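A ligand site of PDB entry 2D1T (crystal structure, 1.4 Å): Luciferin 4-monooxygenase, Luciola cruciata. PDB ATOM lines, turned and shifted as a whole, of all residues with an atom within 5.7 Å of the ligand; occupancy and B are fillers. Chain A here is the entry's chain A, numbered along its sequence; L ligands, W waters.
OD2 of Asp 424 lies within hydrogen-bond range of O6 of the ligand, at 2.6 Å. A nitrogen (N7) of the ligand sits at hydrogen-bond distance from the backbone carbonyl oxygen (O) of Gly 341 (2.8 Å). An oxygen (O4) of the ligand sits at hydrogen-bond distance from a ring nitrogen (NE2) of His 247 (2.8 Å). An oxygen (O3) of the ligand is in hydrogen-bond range of the backbone NH (N) of Thr 345, 3.1 Å away. An oxygen (O3) of the ligand sits at hydrogen-bond distance from the side-chain hydroxyl (OG1) of Thr 345, 2.9 Å away. The backbone NH (N) of Ser 201 sits at hydrogen-bond distance from an oxygen (O4) of the ligand, 3.3 Å away. OG of Ser 201 is in hydrogen-bond range of O4 of the ligand (3.0 Å). The backbone NH (N) of Gly 318 sits at hydrogen-bond distance from a nitrogen (N8) of the ligand (3.1 Å). OE1 of Gln 340 lies within hydrogen-bond range of N7 of the ligand (3.3 Å). The backbone NH (N) of Phe 249 lies close to a sulfur (S1) of the ligand, at 3.7 Å. The side-chain amino group of Lys 531 sits at hydrogen-bond distance from an oxygen (O5) of the ligand (3.4 Å).
The side-chain carboxylate (OD2) of Asp 424 sits at hydrogen-bond distance from the side-chain hydroxyl (OH) of Tyr 342 (2.7 Å). N of Asp 424 lies within hydrogen-bond range of OG1 of Thr 422 (3.0 Å). ND1 of His 247 is in hydrogen-bond range of N of Phe 249 (2.9 Å). NE2 of His 247 is in hydrogen-bond range of OG1 of Thr 529 (3.4 Å). OG1 of Thr 422 lies close to OH of Tyr 342 (3.3 Å). OG of Ser 349 sits close to NE of Arg 220 (3.4 Å). OG of Ser 364 is in hydrogen-bond range of N of Ile 436, at 3.0 Å. The backbone NH (N) of Ser 316 lies within hydrogen-bond range of the backbone carbonyl oxygen (O) of Arg 339, 2.9 Å away.
N6 of the ligand lies close to O of Ala 319 (3.5 Å). Residues that only touch the ligand: Ser 200, Gly 248, Thr 253, Ile 288, Ser 316, Gly 317, Pro 320, Tyr 342, Gly 343, Leu 344, Thr 348, Ser 349, Ala 350, Thr 422, Ile 436 and Arg 439. Hydrophobic or aromatic side chains within 4 Å of the ligand: His 247, Phe 249, Ile 288, Pro 320, Tyr 342, Leu 344, Ala 350 and Ile 436. 26 residues have an atom within 4 Å of the ligand: Ser 200, Ser 201, His 247, Gly 248, Phe 249, Thr 253, Ile 288, Ser 316, Gly 317, Gly 318, Ala 319, Pro 320, Gln 340, Gly 341, Tyr 342, Gly 343, Leu 344, Thr 345, Thr 348, Ser 349, Ala 350, Thr 422, Asp 424, Ile 436, Arg 439 and Lys 531. The nearest printed residue that does not touch the ligand is Ala 315 (4.03 Å).
Water W1 lies within hydrogen-bond range of the backbone carbonyl oxygen (O) of Gly 318 (2.6 Å), the side-chain hydroxyl (OG1) of Thr 529 (2.6 Å), an oxygen (O1) of the ligand (2.7 Å) and the side-chain amino group (NZ) of Lys 531 (2.7 Å). Water W3 lies within hydrogen-bond range of the side-chain carboxylate (OE1) of Glu 346 (2.7 Å) and an oxygen (O3) of the ligand (2.8 Å).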
ATOM      1  N   ASN A 199     -18.009  33.192  -2.625  1.00  0.00           N
ATOM      2  CA  ASN A 199     -18.336  34.014  -3.802  1.00  0.00           C
ATOM      3  C   ASN A 199     -18.221  33.223  -5.091  1.00  0.00           C
ATOM      4  O   ASN A 199     -17.163  32.636  -5.398  1.00  0.00           O
ATOM      5  CB  ASN A 199     -17.371  35.198  -3.949  1.00  0.00           C
ATOM      6  CG  ASN A 199     -17.343  36.141  -2.743  1.00  0.00           C
ATOM      7  OD1 ASN A 199     -18.370  36.386  -2.063  1.00  0.00           O
ATOM      8  ND2 ASN A 199     -16.203  36.720  -2.529  1.00  0.00           N
ATOM      9  N   SER A 200     -19.297  33.257  -5.869  1.00  0.00           N
ATOM     10  CA  SER A 200     -19.252  32.724  -7.225  1.00  0.00           C
ATOM     11  C   SER A 200     -18.309  33.477  -8.136  1.00  0.00           C
ATOM     12  O   SER A 200     -17.954  34.627  -7.893  1.00  0.00           O
ATOM     13  CB  SER A 200     -20.654  32.751  -7.831  1.00  0.00           C
ATOM     14  OG  SER A 200     -21.152  34.064  -7.924  1.00  0.00           O
ATOM     15  N   SER A 201     -17.883  32.809  -9.196  1.00  0.00           N
ATOM     16  CA  SER A 201     -17.105  33.436 -10.252  1.00  0.00           C
ATOM     17  C   SER A 201     -18.019  33.727 -11.430  1.00  0.00           C
ATOM     18  O   SER A 201     -19.065  33.116 -11.596  1.00  0.00           O
ATOM     19  CB  SER A 201     -16.006  32.490 -10.691  1.00  0.00           C
ATOM     20  OG  SER A 201     -16.585  31.221 -10.944  1.00  0.00           O
ATOM     21  N   GLY A 202     -17.608  34.703 -12.238  1.00  0.00           N
ATOM     22  CA  GLY A 202     -18.331  35.055 -13.449  1.00  0.00           C
ATOM     23  C   GLY A 202     -19.677  35.738 -13.275  1.00  0.00           C
ATOM     24  O   GLY A 202     -20.493  35.736 -14.209  1.00  0.00           O
ATOM     25  N   ARG A 220     -21.913  17.144   1.525  1.00  0.00           N
ATOM     26  CA  ARG A 220     -20.819  17.021   0.557  1.00  0.00           C
ATOM     27  C   ARG A 220     -19.879  15.885   0.934  1.00  0.00           C
ATOM     28  O   ARG A 220     -19.414  15.139   0.062  1.00  0.00           O
ATOM     29  CB  ARG A 220     -20.053  18.348   0.442  1.00  0.00           C
ATOM     30  CG  ARG A 220     -18.716  18.204  -0.300  1.00  0.00           C
ATOM     31  CD  ARG A 220     -18.897  17.796  -1.764  1.00  0.00           C
ATOM     32  NE  ARG A 220     -17.624  17.437  -2.373  1.00  0.00           N
ATOM     33  CZ  ARG A 220     -17.505  16.731  -3.502  1.00  0.00           C
ATOM     34  NH1 ARG A 220     -18.594  16.323  -4.153  1.00  0.00           N
ATOM     35  NH2 ARG A 220     -16.312  16.426  -3.967  1.00  0.00           N
ATOM     36  N   HIS A 247     -12.819  29.175  -4.162  1.00  0.00           N
ATOM     37  CA  HIS A 247     -14.072  28.978  -4.878  1.00  0.00           C
ATOM     38  C   HIS A 247     -14.717  27.642  -4.466  1.00  0.00           C
ATOM     39  O   HIS A 247     -14.001  26.697  -4.139  1.00  0.00           O
ATOM     40  CB  HIS A 247     -13.710  28.996  -6.372  1.00  0.00           C
ATOM     41  CG  HIS A 247     -14.871  28.903  -7.297  1.00  0.00           C
ATOM     42  ND1 HIS A 247     -15.478  27.700  -7.596  1.00  0.00           N
ATOM     43  CD2 HIS A 247     -15.519  29.847  -8.019  1.00  0.00           C
ATOM     44  CE1 HIS A 247     -16.460  27.916  -8.453  1.00  0.00           C
ATOM     45  NE2 HIS A 247     -16.517  29.211  -8.716  1.00  0.00           N
ATOM     46  N   GLY A 248     -16.044  27.544  -4.533  1.00  0.00           N
ATOM     47  CA  GLY A 248     -16.723  26.299  -4.169  1.00  0.00           C
ATOM     48  C   GLY A 248     -16.175  25.064  -4.848  1.00  0.00           C
ATOM     49  O   GLY A 248     -16.164  23.978  -4.256  1.00  0.00           O
ATOM     50  N   PHE A 249     -15.779  25.190  -6.112  1.00  0.00           N
ATOM     51  CA  PHE A 249     -15.230  24.039  -6.831  1.00  0.00           C
ATOM     52  C   PHE A 249     -13.940  23.534  -6.125  1.00  0.00           C
ATOM     53  O   PHE A 249     -13.828  22.357  -5.802  1.00  0.00           O
ATOM     54  CB  PHE A 249     -15.037  24.419  -8.308  1.00  0.00           C
ATOM     55  CG  PHE A 249     -14.573  23.308  -9.202  1.00  0.00           C
ATOM     56  CD1 PHE A 249     -14.604  21.961  -8.799  1.00  0.00           C
ATOM     57  CD2 PHE A 249     -14.133  23.597 -10.496  1.00  0.00           C
ATOM     58  CE1 PHE A 249     -14.143  20.936  -9.646  1.00  0.00           C
ATOM     59  CE2 PHE A 249     -13.677  22.574 -11.356  1.00  0.00           C
ATOM     60  CZ  PHE A 249     -13.703  21.242 -10.938  1.00  0.00           C
ATOM     61  N   THR A 253     -14.080  20.136  -3.402  1.00  0.00           N
ATOM     62  CA  THR A 253     -13.273  18.998  -3.833  1.00  0.00           C
ATOM     63  C   THR A 253     -12.136  18.771  -2.843  1.00  0.00           C
ATOM     64  O   THR A 253     -11.940  17.656  -2.374  1.00  0.00           O
ATOM     65  CB  THR A 253     -12.687  19.142  -5.254  1.00  0.00           C
ATOM     66  OG1 THR A 253     -11.991  20.399  -5.398  1.00  0.00           O
ATOM     67  CG2 THR A 253     -13.816  19.123  -6.313  1.00  0.00           C
ATOM     68  N   ILE A 288      -8.258  16.887 -11.107  1.00  0.00           N
ATOM     69  CA  ILE A 288      -9.460  17.706 -11.098  1.00  0.00           C
ATOM     70  C   ILE A 288      -9.123  19.047 -11.734  1.00  0.00           C
ATOM     71  O   ILE A 288      -8.144  19.705 -11.352  1.00  0.00           O
ATOM     72  CB  ILE A 288     -10.046  17.807  -9.674  1.00  0.00           C
ATOM     73  CG1 ILE A 288     -11.377  18.536  -9.678  1.00  0.00           C
ATOM     74  CG2 ILE A 288      -9.074  18.483  -8.686  1.00  0.00           C
ATOM     75  CD1 ILE A 288     -12.493  17.724 -10.323  1.00  0.00           C
ATOM     76  N   ALA A 315     -11.203  14.457 -14.111  1.00  0.00           N
ATOM     77  CA  ALA A 315     -12.508  15.045 -13.830  1.00  0.00           C
ATOM     78  C   ALA A 315     -12.480  16.541 -14.105  1.00  0.00           C
ATOM     79  O   ALA A 315     -11.496  17.225 -13.814  1.00  0.00           O
ATOM     80  CB  ALA A 315     -12.922  14.761 -12.390  1.00  0.00           C
ATOM     81  N   SER A 316     -13.588  17.015 -14.677  1.00  0.00           N
ATOM     82  CA  SER A 316     -13.753  18.406 -15.088  1.00  0.00           C
ATOM     83  C   SER A 316     -14.999  19.018 -14.455  1.00  0.00           C
ATOM     84  O   SER A 316     -15.994  18.320 -14.237  1.00  0.00           O
ATOM     85  CB  SER A 316     -13.921  18.452 -16.606  1.00  0.00           C
ATOM     86  OG  SER A 316     -14.047  19.792 -17.066  1.00  0.00           O
ATOM     87  N   GLY A 317     -14.940  20.313 -14.146  1.00  0.00           N
ATOM     88  CA  GLY A 317     -16.101  21.042 -13.662  1.00  0.00           C
ATOM     89  C   GLY A 317     -15.992  22.531 -13.903  1.00  0.00           C
ATOM     90  O   GLY A 317     -14.964  23.022 -14.396  1.00  0.00           O
ATOM     91  N   GLY A 318     -17.057  23.253 -13.563  1.00  0.00           N
ATOM     92  CA  GLY A 318     -17.044  24.712 -13.541  1.00  0.00           C
ATOM     93  C   GLY A 318     -17.530  25.409 -14.796  1.00  0.00           C
ATOM     94  O   GLY A 318     -17.999  26.542 -14.753  1.00  0.00           O
ATOM     95  N   ALA A 319     -17.421  24.741 -15.945  1.00  0.00           N
ATOM     96  CA  ALA A 319     -17.692  25.392 -17.222  1.00  0.00           C
ATOM     97  C   ALA A 319     -17.988  24.328 -18.240  1.00  0.00           C
ATOM     98  O   ALA A 319     -17.628  23.160 -18.031  1.00  0.00           O
ATOM     99  CB  ALA A 319     -16.520  26.238 -17.641  1.00  0.00           C
ATOM    100  N   PRO A 320     -18.667  24.684 -19.337  1.00  0.00           N
ATOM    101  CA  PRO A 320     -18.967  23.686 -20.365  1.00  0.00           C
ATOM    102  C   PRO A 320     -17.713  23.034 -20.899  1.00  0.00           C
ATOM    103  O   PRO A 320     -16.723  23.695 -21.145  1.00  0.00           O
ATOM    104  CB  PRO A 320     -19.646  24.516 -21.460  1.00  0.00           C
ATOM    105  CG  PRO A 320     -20.284  25.658 -20.711  1.00  0.00           C
ATOM    106  CD  PRO A 320     -19.259  26.000 -19.654  1.00  0.00           C
ATOM    107  N   LEU A 321     -17.778  21.708 -21.048  1.00  0.00           N
ATOM    108  CA  LEU A 321     -16.691  20.950 -21.637  1.00  0.00           C
ATOM    109  C   LEU A 321     -17.163  20.460 -23.012  1.00  0.00           C
ATOM    110  O   LEU A 321     -18.157  19.765 -23.097  1.00  0.00           O
ATOM    111  CB  LEU A 321     -16.370  19.753 -20.746  1.00  0.00           C
ATOM    112  CG  LEU A 321     -15.424  18.720 -21.359  1.00  0.00           C
ATOM    113  CD1 LEU A 321     -14.087  19.333 -21.724  1.00  0.00           C
ATOM    114  CD2 LEU A 321     -15.246  17.548 -20.395  1.00  0.00           C
ATOM    115  N   ARG A 339     -14.630  12.312 -16.398  1.00  0.00           N
ATOM    116  CA  ARG A 339     -15.703  12.461 -15.419  1.00  0.00           C
ATOM    117  C   ARG A 339     -16.027  13.930 -15.258  1.00  0.00           C
ATOM    118  O   ARG A 339     -15.182  14.786 -15.502  1.00  0.00           O
ATOM    119  CB  ARG A 339     -15.288  11.864 -14.086  1.00  0.00           C
ATOM    120  CG  ARG A 339     -15.188  10.346 -14.112  1.00  0.00           C
ATOM    121  CD  ARG A 339     -15.095   9.747 -12.710  1.00  0.00           C
ATOM    122  NE  ARG A 339     -16.389   9.599 -12.043  1.00  0.00           N
ATOM    123  CZ  ARG A 339     -16.551   9.363 -10.735  1.00  0.00           C
ATOM    124  NH1 ARG A 339     -15.488   9.273  -9.931  1.00  0.00           N
ATOM    125  NH2 ARG A 339     -17.771   9.216 -10.218  1.00  0.00           N
ATOM    126  N   GLN A 340     -17.253  14.214 -14.875  1.00  0.00           N
ATOM    127  CA  GLN A 340     -17.669  15.607 -14.742  1.00  0.00           C
ATOM    128  C   GLN A 340     -18.515  15.817 -13.500  1.00  0.00           C
ATOM    129  O   GLN A 340     -19.223  14.901 -13.044  1.00  0.00           O
ATOM    130  CB  GLN A 340     -18.474  15.992 -15.966  1.00  0.00           C
ATOM    131  CG  GLN A 340     -18.526  17.458 -16.235  1.00  0.00           C
ATOM    132  CD  GLN A 340     -18.752  17.832 -17.718  1.00  0.00           C
ATOM    133  OE1 GLN A 340     -18.784  18.990 -18.001  1.00  0.00           O
ATOM    134  NE2 GLN A 340     -18.940  16.857 -18.612  1.00  0.00           N
ATOM    135  N   GLY A 341     -18.427  17.027 -12.968  1.00  0.00           N
ATOM    136  CA  GLY A 341     -19.384  17.508 -11.982  1.00  0.00           C
ATOM    137  C   GLY A 341     -19.883  18.885 -12.354  1.00  0.00           C
ATOM    138  O   GLY A 341     -19.153  19.672 -12.957  1.00  0.00           O
ATOM    139  N   TYR A 342     -21.117  19.163 -11.969  1.00  0.00           N
ATOM    140  CA  TYR A 342     -21.775  20.440 -12.218  1.00  0.00           C
ATOM    141  C   TYR A 342     -22.439  20.894 -10.943  1.00  0.00           C
ATOM    142  O   TYR A 342     -23.206  20.127 -10.320  1.00  0.00           O
ATOM    143  CB  TYR A 342     -22.831  20.260 -13.336  1.00  0.00           C
ATOM    144  CG  TYR A 342     -23.968  21.273 -13.336  1.00  0.00           C
ATOM    145  CD1 TYR A 342     -23.804  22.561 -13.853  1.00  0.00           C
ATOM    146  CD2 TYR A 342     -25.215  20.928 -12.825  1.00  0.00           C
ATOM    147  CE1 TYR A 342     -24.861  23.482 -13.833  1.00  0.00           C
ATOM    148  CE2 TYR A 342     -26.286  21.832 -12.810  1.00  0.00           C
ATOM    149  CZ  TYR A 342     -26.092  23.093 -13.344  1.00  0.00           C
ATOM    150  OH  TYR A 342     -27.133  23.967 -13.356  1.00  0.00           O
ATOM    151  N   GLY A 343     -22.122  22.112 -10.547  1.00  0.00           N
ATOM    152  CA  GLY A 343     -22.773  22.716  -9.401  1.00  0.00           C
ATOM    153  C   GLY A 343     -22.660  24.212  -9.431  1.00  0.00           C
ATOM    154  O   GLY A 343     -22.117  24.789 -10.387  1.00  0.00           O
ATOM    155  N   LEU A 344     -23.247  24.818  -8.414  1.00  0.00           N
ATOM    156  CA  LEU A 344     -23.190  26.267  -8.225  1.00  0.00           C
ATOM    157  C   LEU A 344     -22.677  26.569  -6.821  1.00  0.00           C
ATOM    158  O   LEU A 344     -22.830  25.768  -5.916  1.00  0.00           O
ATOM    159  CB  LEU A 344     -24.597  26.869  -8.343  1.00  0.00           C
ATOM    160  CG  LEU A 344     -25.257  26.950  -9.727  1.00  0.00           C
ATOM    161  CD1 LEU A 344     -25.733  25.581 -10.267  1.00  0.00           C
ATOM    162  CD2 LEU A 344     -26.432  27.918  -9.665  1.00  0.00           C
ATOM    163  N   THR A 345     -22.115  27.755  -6.630  1.00  0.00           N
ATOM    164  CA  THR A 345     -21.717  28.118  -5.268  1.00  0.00           C
ATOM    165  C   THR A 345     -22.907  27.937  -4.294  1.00  0.00           C
ATOM    166  O   THR A 345     -22.739  27.415  -3.192  1.00  0.00           O
ATOM    167  CB  THR A 345     -21.246  29.575  -5.265  1.00  0.00           C
ATOM    168  OG1 THR A 345     -20.183  29.729  -6.205  1.00  0.00           O
ATOM    169  CG2 THR A 345     -20.649  29.958  -3.892  1.00  0.00           C
ATOM    170  N   GLU A 346     -24.094  28.302  -4.765  1.00  0.00           N
ATOM    171  CA  GLU A 346     -25.322  28.249  -3.971  1.00  0.00           C
ATOM    172  C   GLU A 346     -25.828  26.811  -3.729  1.00  0.00           C
ATOM    173  O   GLU A 346     -26.750  26.634  -2.909  1.00  0.00           O
ATOM    174  CB  GLU A 346     -26.413  29.087  -4.652  1.00  0.00           C
ATOM    175  CG  GLU A 346     -26.075  30.568  -4.720  1.00  0.00           C
ATOM    176  CD  GLU A 346     -25.396  30.984  -6.019  1.00  0.00           C
ATOM    177  OE1 GLU A 346     -24.770  30.142  -6.703  1.00  0.00           O
ATOM    178  OE2 GLU A 346     -25.461  32.177  -6.366  1.00  0.00           O
ATOM    179  N   THR A 348     -23.512  24.481  -2.768  1.00  0.00           N
ATOM    180  CA  THR A 348     -22.298  23.999  -2.080  1.00  0.00           C
ATOM    181  C   THR A 348     -21.277  23.401  -3.034  1.00  0.00           C
ATOM    182  O   THR A 348     -20.169  23.935  -3.228  1.00  0.00           O
ATOM    183  CB  THR A 348     -22.647  22.981  -0.955  1.00  0.00           C
ATOM    184  OG1 THR A 348     -23.556  23.607  -0.036  1.00  0.00           O
ATOM    185  CG2 THR A 348     -21.403  22.666  -0.111  1.00  0.00           C
ATOM    186  N   SER A 349     -21.667  22.280  -3.631  1.00  0.00           N
ATOM    187  CA  SER A 349     -20.787  21.538  -4.518  1.00  0.00           C
ATOM    188  C   SER A 349     -21.566  21.005  -5.713  1.00  0.00           C
ATOM    189  O   SER A 349     -22.685  21.481  -6.007  1.00  0.00           O
ATOM    190  CB  SER A 349     -20.104  20.399  -3.719  1.00  0.00           C
ATOM    191  OG  SER A 349     -19.053  19.782  -4.448  1.00  0.00           O
ATOM    192  N   ALA A 350     -20.986  20.036  -6.407  1.00  0.00           N
ATOM    193  CA  ALA A 350     -21.645  19.435  -7.557  1.00  0.00           C
ATOM    194  C   ALA A 350     -22.913  18.691  -7.142  1.00  0.00           C
ATOM    195  O   ALA A 350     -22.878  17.898  -6.200  1.00  0.00           O
ATOM    196  CB  ALA A 350     -20.691  18.484  -8.277  1.00  0.00           C
ATOM    197  N   ILE A 353     -23.246  14.645 -11.140  1.00  0.00           N
ATOM    198  CA  ILE A 353     -21.888  14.082 -11.260  1.00  0.00           C
ATOM    199  C   ILE A 353     -21.976  12.806 -12.107  1.00  0.00           C
ATOM    200  O   ILE A 353     -22.924  12.030 -11.946  1.00  0.00           O
ATOM    201  CB  ILE A 353     -21.321  13.739  -9.879  1.00  0.00           C
ATOM    202  CG1 ILE A 353     -21.102  15.007  -9.059  1.00  0.00           C
ATOM    203  CG2 ILE A 353     -19.975  12.974 -10.013  1.00  0.00           C
ATOM    204  CD1 ILE A 353     -20.662  14.764  -7.607  1.00  0.00           C
ATOM    205  N   SER A 364     -23.362  15.450 -18.623  1.00  0.00           N
ATOM    206  CA  SER A 364     -22.828  16.087 -17.438  1.00  0.00           C
ATOM    207  C   SER A 364     -22.846  15.142 -16.202  1.00  0.00           C
ATOM    208  O   SER A 364     -22.037  15.289 -15.295  1.00  0.00           O
ATOM    209  CB  SER A 364     -23.575  17.402 -17.166  1.00  0.00           C
ATOM    210  OG  SER A 364     -23.452  18.296 -18.277  1.00  0.00           O
ATOM    211  N   THR A 422     -31.245  27.378 -11.442  1.00  0.00           N
ATOM    212  CA  THR A 422     -29.801  27.509 -11.693  1.00  0.00           C
ATOM    213  C   THR A 422     -29.405  28.592 -12.655  1.00  0.00           C
ATOM    214  O   THR A 422     -28.268  29.017 -12.646  1.00  0.00           O
ATOM    215  CB  THR A 422     -29.214  26.210 -12.235  1.00  0.00           C
ATOM    216  OG1 THR A 422     -29.804  25.918 -13.518  1.00  0.00           O
ATOM    217  CG2 THR A 422     -29.500  25.040 -11.319  1.00  0.00           C
ATOM    218  N   GLY A 423     -30.331  29.017 -13.509  1.00  0.00           N
ATOM    219  CA  GLY A 423     -29.989  29.924 -14.603  1.00  0.00           C
ATOM    220  C   GLY A 423     -29.312  29.204 -15.757  1.00  0.00           C
ATOM    221  O   GLY A 423     -28.867  29.879 -16.692  1.00  0.00           O
ATOM    222  N   ASP A 424     -29.256  27.876 -15.724  1.00  0.00           N
ATOM    223  CA  ASP A 424     -28.639  27.115 -16.797  1.00  0.00           C
ATOM    224  C   ASP A 424     -29.650  26.371 -17.654  1.00  0.00           C
ATOM    225  O   ASP A 424     -30.659  25.865 -17.140  1.00  0.00           O
ATOM    226  CB  ASP A 424     -27.683  26.076 -16.231  1.00  0.00           C
ATOM    227  CG  ASP A 424     -26.575  26.707 -15.442  1.00  0.00           C
ATOM    228  OD1 ASP A 424     -25.959  27.671 -15.943  1.00  0.00           O
ATOM    229  OD2 ASP A 424     -26.293  26.314 -14.313  1.00  0.00           O
ATOM    230  N   ILE A 436     -25.772  19.728 -19.434  1.00  0.00           N
ATOM    231  CA  ILE A 436     -25.827  21.149 -19.210  1.00  0.00           C
ATOM    232  C   ILE A 436     -25.228  21.844 -20.419  1.00  0.00           C
ATOM    233  O   ILE A 436     -24.074  21.604 -20.787  1.00  0.00           O
ATOM    234  CB  ILE A 436     -25.056  21.532 -17.920  1.00  0.00           C
ATOM    235  CG1 ILE A 436     -25.538  20.708 -16.713  1.00  0.00           C
ATOM    236  CG2 ILE A 436     -25.106  23.045 -17.651  1.00  0.00           C
ATOM    237  CD1 ILE A 436     -27.023  20.906 -16.326  1.00  0.00           C
ATOM    238  N   ASP A 438     -25.488  25.580 -21.424  1.00  0.00           N
ATOM    239  CA  ASP A 438     -24.856  26.887 -21.196  1.00  0.00           C
ATOM    240  C   ASP A 438     -25.769  27.652 -20.268  1.00  0.00           C
ATOM    241  O   ASP A 438     -26.828  27.165 -19.869  1.00  0.00           O
ATOM    242  CB  ASP A 438     -24.697  27.641 -22.525  1.00  0.00           C
ATOM    243  CG  ASP A 438     -23.499  28.572 -22.534  1.00  0.00           C
ATOM    244  OD1 ASP A 438     -23.106  29.152 -21.492  1.00  0.00           O
ATOM    245  OD2 ASP A 438     -22.862  28.802 -23.589  1.00  0.00           O
ATOM    246  N   ARG A 439     -25.372  28.863 -19.939  1.00  0.00           N
ATOM    247  CA  ARG A 439     -26.182  29.752 -19.128  1.00  0.00           C
ATOM    248  C   ARG A 439     -27.268  30.397 -19.961  1.00  0.00           C
ATOM    249  O   ARG A 439     -27.023  30.846 -21.075  1.00  0.00           O
ATOM    250  CB  ARG A 439     -25.294  30.817 -18.475  1.00  0.00           C
ATOM    251  CG  ARG A 439     -24.375  30.247 -17.416  1.00  0.00           C
ATOM    252  CD  ARG A 439     -23.272  31.177 -16.988  1.00  0.00           C
ATOM    253  NE  ARG A 439     -22.292  31.405 -18.051  1.00  0.00           N
ATOM    254  CZ  ARG A 439     -21.385  32.385 -18.059  1.00  0.00           C
ATOM    255  NH1 ARG A 439     -21.298  33.214 -17.014  1.00  0.00           N
ATOM    256  NH2 ARG A 439     -20.548  32.514 -19.076  1.00  0.00           N
ATOM    257  N   THR A 529     -13.176  30.397 -12.928  1.00  0.00           N
ATOM    258  CA  THR A 529     -13.358  28.958 -13.201  1.00  0.00           C
ATOM    259  C   THR A 529     -13.815  28.719 -14.642  1.00  0.00           C
ATOM    260  O   THR A 529     -14.531  27.742 -14.918  1.00  0.00           O
ATOM    261  CB  THR A 529     -14.309  28.278 -12.204  1.00  0.00           C
ATOM    262  OG1 THR A 529     -15.463  29.111 -11.994  1.00  0.00           O
ATOM    263  CG2 THR A 529     -13.665  28.167 -10.817  1.00  0.00           C
ATOM    264  N   LYS A 531     -15.664  30.377 -17.071  1.00  0.00           N
ATOM    265  CA  LYS A 531     -16.887  30.768 -17.771  1.00  0.00           C
ATOM    266  C   LYS A 531     -16.604  32.032 -18.577  1.00  0.00           C
ATOM    267  O   LYS A 531     -15.915  32.957 -18.087  1.00  0.00           O
ATOM    268  CB  LYS A 531     -18.037  30.999 -16.784  1.00  0.00           C
ATOM    269  CG  LYS A 531     -18.356  29.747 -15.976  1.00  0.00           C
ATOM    270  CD  LYS A 531     -19.682  29.888 -15.209  1.00  0.00           C
ATOM    271  CE  LYS A 531     -19.672  30.956 -14.121  1.00  0.00           C
ATOM    272  NZ  LYS A 531     -18.611  30.740 -13.088  1.00  0.00           N
HETATM  273  O1  LIG L   1     -19.002  26.573 -10.909  1.00  0.00           O
HETATM  274  C1  LIG L   1     -19.423  26.565  -9.762  1.00  0.00           C
HETATM  275  C2  LIG L   1     -19.215  25.373  -8.930  1.00  0.00           C
HETATM  276  N1  LIG L   1     -18.776  24.202  -9.450  1.00  0.00           N
HETATM  277  C3  LIG L   1     -19.436  25.332  -7.556  1.00  0.00           C
HETATM  278  S1  LIG L   1     -19.066  23.802  -6.921  1.00  0.00           S
HETATM  279  C4  LIG L   1     -18.709  23.291  -8.502  1.00  0.00           C
HETATM  280  C5  LIG L   1     -18.251  21.893  -8.818  1.00  0.00           C
HETATM  281  S2  LIG L   1     -17.884  21.408 -10.423  1.00  0.00           S
HETATM  282  C6  LIG L   1     -17.347  19.948  -9.794  1.00  0.00           C
HETATM  283  C7  LIG L   1     -16.808  18.837 -10.478  1.00  0.00           C
HETATM  284  C8  LIG L   1     -16.404  17.698  -9.730  1.00  0.00           C
HETATM  285  O2  LIG L   1     -15.896  16.606 -10.382  1.00  0.00           O
HETATM  286  C9  LIG L   1     -17.395  19.911  -8.314  1.00  0.00           C
HETATM  287  N2  LIG L   1     -17.858  21.083  -7.831  1.00  0.00           N
HETATM  288  C10 LIG L   1     -16.982  18.767  -7.641  1.00  0.00           C
HETATM  289  C11 LIG L   1     -16.476  17.676  -8.339  1.00  0.00           C
HETATM  290  N3  LIG L   1     -19.998  27.563  -9.104  1.00  0.00           N
HETATM  291  S3  LIG L   1     -20.206  29.022  -9.743  1.00  0.00           S
HETATM  292  O3  LIG L   1     -21.249  29.670  -8.950  1.00  0.00           O
HETATM  293  O4  LIG L   1     -19.050  29.840  -9.847  1.00  0.00           O
HETATM  294  O5  LIG L   1     -20.766  28.909 -11.235  1.00  0.00           O
HETATM  295  C12 LIG L   1     -21.881  28.051 -11.420  1.00  0.00           C
HETATM  296  C13 LIG L   1     -22.106  27.981 -12.909  1.00  0.00           C
HETATM  297  C14 LIG L   1     -23.272  27.084 -13.282  1.00  0.00           C
HETATM  298  O6  LIG L   1     -24.523  27.759 -13.072  1.00  0.00           O
HETATM  299  C15 LIG L   1     -22.958  26.682 -14.708  1.00  0.00           C
HETATM  300  O7  LIG L   1     -23.302  27.773 -15.561  1.00  0.00           O
HETATM  301  C16 LIG L   1     -21.444  26.596 -14.644  1.00  0.00           C
HETATM  302  O8  LIG L   1     -21.001  27.312 -13.506  1.00  0.00           O
HETATM  303  N4  LIG L   1     -20.982  25.195 -14.510  1.00  0.00           N
HETATM  304  C17 LIG L   1     -20.989  24.347 -15.515  1.00  0.00           C
HETATM  305  N5  LIG L   1     -21.399  24.424 -16.783  1.00  0.00           N
HETATM  306  C18 LIG L   1     -21.297  23.346 -17.562  1.00  0.00           C
HETATM  307  N6  LIG L   1     -20.807  22.164 -17.131  1.00  0.00           N
HETATM  308  C19 LIG L   1     -20.463  23.112 -14.976  1.00  0.00           C
HETATM  309  C20 LIG L   1     -20.363  21.959 -15.876  1.00  0.00           C
HETATM  310  N7  LIG L   1     -19.884  20.765 -15.473  1.00  0.00           N
HETATM  311  N8  LIG L   1     -20.162  23.277 -13.683  1.00  0.00           N
HETATM  312  C21 LIG L   1     -20.461  24.559 -13.416  1.00  0.00           C
HETATM  313  O   HOH W   1     -17.815  28.170 -12.703  1.00  0.00           O
HETATM  314  O   HOH W   2     -14.923  14.561  -8.895  1.00  0.00           O
HETATM  315  O   HOH W   3     -23.830  30.638  -9.224  1.00  0.00           O
HETATM  316  O   HOH W   4     -17.040  21.374  -5.158  1.00  0.00           O
HETATM  317  O   HOH W   5     -16.232  13.362 -10.667  1.00  0.00           O
HETATM  318  O   HOH W   6     -26.459  30.159 -14.521  1.00  0.00           O
HETATM  319  O   HOH W   7     -24.822  30.330 -11.817  1.00  0.00           O
HETATM  320  O   HOH W   8     -22.402  26.852 -18.037  1.00  0.00           O
